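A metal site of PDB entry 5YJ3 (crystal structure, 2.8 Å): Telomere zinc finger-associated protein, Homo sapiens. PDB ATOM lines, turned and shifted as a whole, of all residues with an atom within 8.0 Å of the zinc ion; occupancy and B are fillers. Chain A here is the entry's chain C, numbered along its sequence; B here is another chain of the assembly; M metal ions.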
ATOM      1  N   GLU A  66      10.480  -6.796 -35.556  1.00  0.00           N
ATOM      2  CA  GLU A  66       9.242  -6.214 -35.048  1.00  0.00           C
ATOM      3  C   GLU A  66       8.764  -6.983 -33.823  1.00  0.00           C
ATOM      4  O   GLU A  66       8.728  -8.223 -33.823  1.00  0.00           O
ATOM      5  CB  GLU A  66       8.148  -6.225 -36.123  1.00  0.00           C
ATOM      6  CG  GLU A  66       6.771  -5.851 -35.581  1.00  0.00           C
ATOM      7  CD  GLU A  66       5.687  -5.937 -36.635  1.00  0.00           C
ATOM      8  OE1 GLU A  66       5.988  -5.685 -37.824  1.00  0.00           O
ATOM      9  OE2 GLU A  66       4.532  -6.257 -36.283  1.00  0.00           O
ATOM     10  N   CYS A  67       8.380  -6.246 -32.792  1.00  0.00           N
ATOM     11  CA  CYS A  67       7.707  -6.839 -31.649  1.00  0.00           C
ATOM     12  C   CYS A  67       6.293  -7.242 -32.036  1.00  0.00           C
ATOM     13  O   CYS A  67       5.511  -6.427 -32.527  1.00  0.00           O
ATOM     14  CB  CYS A  67       7.664  -5.868 -30.483  1.00  0.00           C
ATOM     15  SG  CYS A  67       6.515  -6.354 -29.201  1.00  0.00           S
ATOM     16  N   THR A  68       5.951  -8.518 -31.814  1.00  0.00           N
ATOM     17  CA  THR A  68       4.594  -8.956 -32.100  1.00  0.00           C
ATOM     18  C   THR A  68       3.584  -8.389 -31.115  1.00  0.00           C
ATOM     19  O   THR A  68       2.396  -8.325 -31.444  1.00  0.00           O
ATOM     20  CB  THR A  68       4.513 -10.484 -32.088  1.00  0.00           C
ATOM     21  OG1 THR A  68       5.215 -10.995 -30.947  1.00  0.00           O
ATOM     22  CG2 THR A  68       5.122 -11.060 -33.358  1.00  0.00           C
ATOM     23  N   GLU A  69       4.019  -7.983 -29.921  1.00  0.00           N
ATOM     24  CA  GLU A  69       3.064  -7.516 -28.911  1.00  0.00           C
ATOM     25  C   GLU A  69       2.643  -6.067 -29.158  1.00  0.00           C
ATOM     26  O   GLU A  69       1.458  -5.740 -29.076  1.00  0.00           O
ATOM     27  CB  GLU A  69       3.647  -7.662 -27.506  1.00  0.00           C
ATOM     28  CG  GLU A  69       3.506  -9.055 -26.899  1.00  0.00           C
ATOM     29  CD  GLU A  69       3.243  -9.015 -25.397  1.00  0.00           C
ATOM     30  OE1 GLU A  69       2.806  -7.960 -24.900  1.00  0.00           O
ATOM     31  OE2 GLU A  69       3.470 -10.052 -24.719  1.00  0.00           O
ATOM     32  N   CYS A  70       3.601  -5.179 -29.444  1.00  0.00           N
ATOM     33  CA  CYS A  70       3.310  -3.760 -29.578  1.00  0.00           C
ATOM     34  C   CYS A  70       3.748  -3.169 -30.913  1.00  0.00           C
ATOM     35  O   CYS A  70       3.623  -1.951 -31.115  1.00  0.00           O
ATOM     36  CB  CYS A  70       3.961  -2.972 -28.448  1.00  0.00           C
ATOM     37  SG  CYS A  70       5.748  -2.872 -28.596  1.00  0.00           S
ATOM     38  N   GLY A  71       4.272  -3.986 -31.829  1.00  0.00           N
ATOM     39  CA  GLY A  71       4.574  -3.509 -33.172  1.00  0.00           C
ATOM     40  C   GLY A  71       5.795  -2.632 -33.296  1.00  0.00           C
ATOM     41  O   GLY A  71       6.017  -2.049 -34.366  1.00  0.00           O
ATOM     42  N   TYR A  72       6.594  -2.501 -32.249  1.00  0.00           N
ATOM     43  CA  TYR A  72       7.817  -1.725 -32.338  1.00  0.00           C
ATOM     44  C   TYR A  72       8.839  -2.485 -33.171  1.00  0.00           C
ATOM     45  O   TYR A  72       9.039  -3.686 -32.979  1.00  0.00           O
ATOM     46  CB  TYR A  72       8.379  -1.443 -30.949  1.00  0.00           C
ATOM     47  CG  TYR A  72       9.351  -0.291 -30.902  1.00  0.00           C
ATOM     48  CD1 TYR A  72      10.650  -0.441 -31.368  1.00  0.00           C
ATOM     49  CD2 TYR A  72       8.982   0.947 -30.378  1.00  0.00           C
ATOM     50  CE1 TYR A  72      11.538   0.608 -31.320  1.00  0.00           C
ATOM     51  CE2 TYR A  72       9.871   1.997 -30.329  1.00  0.00           C
ATOM     52  CZ  TYR A  72      11.151   1.825 -30.804  1.00  0.00           C
ATOM     53  OH  TYR A  72      12.039   2.874 -30.755  1.00  0.00           O
ATOM     54  N   LYS A  73       9.495  -1.785 -34.088  1.00  0.00           N
ATOM     55  CA  LYS A  73      10.474  -2.386 -34.983  1.00  0.00           C
ATOM     56  C   LYS A  73      11.872  -1.989 -34.531  1.00  0.00           C
ATOM     57  O   LYS A  73      12.157  -0.802 -34.345  1.00  0.00           O
ATOM     58  CB  LYS A  73      10.231  -1.960 -36.428  1.00  0.00           C
ATOM     59  CG  LYS A  73       8.833  -2.284 -36.920  1.00  0.00           C
ATOM     60  CD  LYS A  73       8.674  -2.043 -38.411  1.00  0.00           C
ATOM     61  CE  LYS A  73       9.596  -2.956 -39.215  1.00  0.00           C
ATOM     62  NZ  LYS A  73       9.428  -2.765 -40.673  1.00  0.00           N
ATOM     63  N   PHE A  74      12.744  -2.983 -34.350  1.00  0.00           N
ATOM     64  CA  PHE A  74      14.082  -2.773 -33.820  1.00  0.00           C
ATOM     65  C   PHE A  74      15.144  -3.008 -34.887  1.00  0.00           C
ATOM     66  O   PHE A  74      14.907  -3.651 -35.910  1.00  0.00           O
ATOM     67  CB  PHE A  74      14.345  -3.706 -32.632  1.00  0.00           C
ATOM     68  CG  PHE A  74      13.538  -3.370 -31.423  1.00  0.00           C
ATOM     69  CD1 PHE A  74      12.277  -3.907 -31.247  1.00  0.00           C
ATOM     70  CD2 PHE A  74      14.024  -2.502 -30.464  1.00  0.00           C
ATOM     71  CE1 PHE A  74      11.517  -3.583 -30.138  1.00  0.00           C
ATOM     72  CE2 PHE A  74      13.282  -2.179 -29.346  1.00  0.00           C
ATOM     73  CZ  PHE A  74      12.032  -2.718 -29.189  1.00  0.00           C
ATOM     74  N   LEU A  80      15.260  -6.523 -29.518  1.00  0.00           N
ATOM     75  CA  LEU A  80      13.906  -7.022 -29.439  1.00  0.00           C
ATOM     76  C   LEU A  80      13.734  -7.993 -28.283  1.00  0.00           C
ATOM     77  O   LEU A  80      12.696  -7.984 -27.612  1.00  0.00           O
ATOM     78  CB  LEU A  80      13.492  -7.693 -30.751  1.00  0.00           C
ATOM     79  CG  LEU A  80      12.086  -8.310 -30.724  1.00  0.00           C
ATOM     80  CD1 LEU A  80      11.064  -7.261 -30.316  1.00  0.00           C
ATOM     81  CD2 LEU A  80      11.721  -8.915 -32.059  1.00  0.00           C
ATOM     82  N   HIS A  83      13.723  -5.951 -25.252  1.00  0.00           N
ATOM     83  CA  HIS A  83      12.419  -5.300 -25.220  1.00  0.00           C
ATOM     84  C   HIS A  83      11.353  -6.234 -24.673  1.00  0.00           C
ATOM     85  O   HIS A  83      10.575  -5.849 -23.787  1.00  0.00           O
ATOM     86  CB  HIS A  83      12.048  -4.844 -26.625  1.00  0.00           C
ATOM     87  CG  HIS A  83      10.616  -4.441 -26.773  1.00  0.00           C
ATOM     88  ND1 HIS A  83      10.035  -3.442 -26.013  1.00  0.00           N
ATOM     89  CD2 HIS A  83       9.634  -4.886 -27.594  1.00  0.00           C
ATOM     90  CE1 HIS A  83       8.776  -3.302 -26.359  1.00  0.00           C
ATOM     91  NE2 HIS A  83       8.500  -4.170 -27.318  1.00  0.00           N
ATOM     92  N   MET A  84      11.306  -7.466 -25.182  1.00  0.00           N
ATOM     93  CA  MET A  84      10.314  -8.426 -24.723  1.00  0.00           C
ATOM     94  C   MET A  84      10.404  -8.620 -23.211  1.00  0.00           C
ATOM     95  O   MET A  84       9.375  -8.853 -22.560  1.00  0.00           O
ATOM     96  CB  MET A  84      10.507  -9.761 -25.443  1.00  0.00           C
ATOM     97  CG  MET A  84      10.201  -9.703 -26.924  1.00  0.00           C
ATOM     98  SD  MET A  84       8.525  -9.158 -27.266  1.00  0.00           S
ATOM     99  CE  MET A  84       8.334  -9.668 -28.970  1.00  0.00           C
ATOM    100  N   ILE A  86      10.373  -6.547 -21.127  1.00  0.00           N
ATOM    101  CA  ILE A  86       9.593  -5.496 -20.482  1.00  0.00           C
ATOM    102  C   ILE A  86       8.116  -5.873 -20.429  1.00  0.00           C
ATOM    103  O   ILE A  86       7.482  -5.779 -19.378  1.00  0.00           O
ATOM    104  CB  ILE A  86       9.802  -4.155 -21.204  1.00  0.00           C
ATOM    105  CG1 ILE A  86      11.250  -3.701 -21.070  1.00  0.00           C
ATOM    106  CG2 ILE A  86       8.853  -3.108 -20.627  1.00  0.00           C
ATOM    107  CD1 ILE A  86      11.658  -3.389 -19.656  1.00  0.00           C
ATOM    108  N   HIS A  87       7.548  -6.280 -21.575  1.00  0.00           N
ATOM    109  CA  HIS A  87       6.201  -6.833 -21.588  1.00  0.00           C
ATOM    110  C   HIS A  87       6.033  -7.957 -20.578  1.00  0.00           C
ATOM    111  O   HIS A  87       4.922  -8.256 -20.161  1.00  0.00           O
ATOM    112  CB  HIS A  87       5.842  -7.345 -22.989  1.00  0.00           C
ATOM    113  CG  HIS A  87       5.763  -6.275 -24.034  1.00  0.00           C
ATOM    114  ND1 HIS A  87       4.811  -5.279 -24.001  1.00  0.00           N
ATOM    115  CD2 HIS A  87       6.510  -6.052 -25.132  1.00  0.00           C
ATOM    116  CE1 HIS A  87       4.982  -4.482 -25.040  1.00  0.00           C
ATOM    117  NE2 HIS A  87       6.002  -4.933 -25.747  1.00  0.00           N
ATOM    118  N   TYR A  93       2.217  -2.067 -22.439  1.00  0.00           N
ATOM    119  CA  TYR A  93       3.429  -1.334 -22.764  1.00  0.00           C
ATOM    120  C   TYR A  93       3.472  -1.058 -24.261  1.00  0.00           C
ATOM    121  O   TYR A  93       3.339  -1.975 -25.072  1.00  0.00           O
ATOM    122  CB  TYR A  93       4.657  -2.111 -22.317  1.00  0.00           C
ATOM    123  CG  TYR A  93       5.980  -1.426 -22.596  1.00  0.00           C
ATOM    124  CD1 TYR A  93       6.290  -0.197 -22.040  1.00  0.00           C
ATOM    125  CD2 TYR A  93       6.932  -2.031 -23.407  1.00  0.00           C
ATOM    126  CE1 TYR A  93       7.504   0.421 -22.292  1.00  0.00           C
ATOM    127  CE2 TYR A  93       8.152  -1.432 -23.668  1.00  0.00           C
ATOM    128  CZ  TYR A  93       8.424  -0.201 -23.109  1.00  0.00           C
ATOM    129  OH  TYR A  93       9.644   0.398 -23.370  1.00  0.00           O
ATOM    130  N   ASN A  94       3.652   0.207 -24.623  1.00  0.00           N
ATOM    131  CA  ASN A  94       3.702   0.613 -26.033  1.00  0.00           C
ATOM    132  C   ASN A  94       4.580   1.842 -26.140  1.00  0.00           C
ATOM    133  O   ASN A  94       4.090   2.978 -26.177  1.00  0.00           O
ATOM    134  CB  ASN A  94       2.308   0.877 -26.580  1.00  0.00           C
ATOM    135  CG  ASN A  94       2.264   0.924 -28.092  1.00  0.00           C
ATOM    136  OD1 ASN A  94       3.260   0.636 -28.756  1.00  0.00           O
ATOM    137  ND2 ASN A  94       1.110   1.280 -28.650  1.00  0.00           N
ATOM    138  N   PRO A  95       5.903   1.661 -26.196  1.00  0.00           N
ATOM    139  CA  PRO A  95       6.816   2.807 -26.109  1.00  0.00           C
ATOM    140  C   PRO A  95       6.871   3.597 -27.404  1.00  0.00           C
ATOM    141  O   PRO A  95       6.559   3.111 -28.493  1.00  0.00           O
ATOM    142  CB  PRO A  95       8.161   2.141 -25.800  1.00  0.00           C
ATOM    143  CG  PRO A  95       8.056   0.802 -26.430  1.00  0.00           C
ATOM    144  CD  PRO A  95       6.615   0.383 -26.281  1.00  0.00           C
ATOM    145  P    DA B  17      12.841  -0.840 -24.683  1.00  0.00           P
ATOM    146  OP1  DA B  17      11.398  -1.068 -24.900  1.00  0.00           O
ATOM    147  OP2  DA B  17      13.706  -1.960 -24.258  1.00  0.00           O
ATOM    148  O5'  DA B  17      13.447  -0.217 -26.027  1.00  0.00           O
ATOM    149  C5'  DA B  17      12.860   0.949 -26.585  1.00  0.00           C
ATOM    150  C4'  DA B  17      13.909   1.839 -27.221  1.00  0.00           C
ATOM    151  O4'  DA B  17      14.923   2.170 -26.240  1.00  0.00           O
ATOM    152  C3'  DA B  17      14.659   1.231 -28.397  1.00  0.00           C
ATOM    153  O3'  DA B  17      14.943   2.240 -29.350  1.00  0.00           O
ATOM    154  C2'  DA B  17      15.940   0.718 -27.743  1.00  0.00           C
ATOM    155  C1'  DA B  17      16.189   1.826 -26.732  1.00  0.00           C
ATOM    156  N9   DA B  17      17.026   1.418 -25.602  1.00  0.00           N
ATOM    157  C8   DA B  17      16.710   0.511 -24.635  1.00  0.00           C
ATOM    158  N7   DA B  17      17.642   0.369 -23.719  1.00  0.00           N
ATOM    159  C5   DA B  17      18.625   1.264 -24.107  1.00  0.00           C
ATOM    160  C6   DA B  17      19.866   1.596 -23.546  1.00  0.00           C
ATOM    161  N6   DA B  17      20.360   1.036 -22.448  1.00  0.00           N
ATOM    162  N1   DA B  17      20.609   2.533 -24.176  1.00  0.00           N
ATOM    163  C2   DA B  17      20.113   3.096 -25.291  1.00  0.00           C
ATOM    164  N3   DA B  17      18.956   2.871 -25.911  1.00  0.00           N
ATOM    165  C4   DA B  17      18.259   1.928 -25.263  1.00  0.00           C
HETATM  166 ZN    ZN M   1       6.710  -4.681 -27.720  1.00  0.00          ZN
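Four residues have an atom within 4 Å of the zinc ion: Cys 67, Cys 70, His 83 and His 87.
The nearest printed residue that does not touch the zinc ion is Glu 69 (4.3 Å).
OP1 of DA 17 of chain B lies within hydrogen-bond range of ND1 of His 83 (3.0 Å).
ND1 of His 87 sits at hydrogen-bond distance from OE1 of Glu 69 (3.5 Å).
The backbone NH (N) of Tyr 72 lies close to the side-chain sulfur (SG) of Cys 70 (3.8 Å).
The side-chain sulfur (SG) of Cys 67 sits close to the backbone NH (N) of Glu 69 (3.1 Å).
The backbone NH of Cys 67 sits at hydrogen-bond distance from the backbone carbonyl oxygen of Tyr 72 (2.7 Å).
The zinc ion is bound by a ring nitrogen (NE2) of His 83 (1.9 Å), a ring nitrogen (NE2) of His 87 (2.1 Å), the side-chain sulfur (SG) of Cys 70 (2.2 Å) and the side-chain sulfur (SG) of Cys 67 (2.2 Å).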
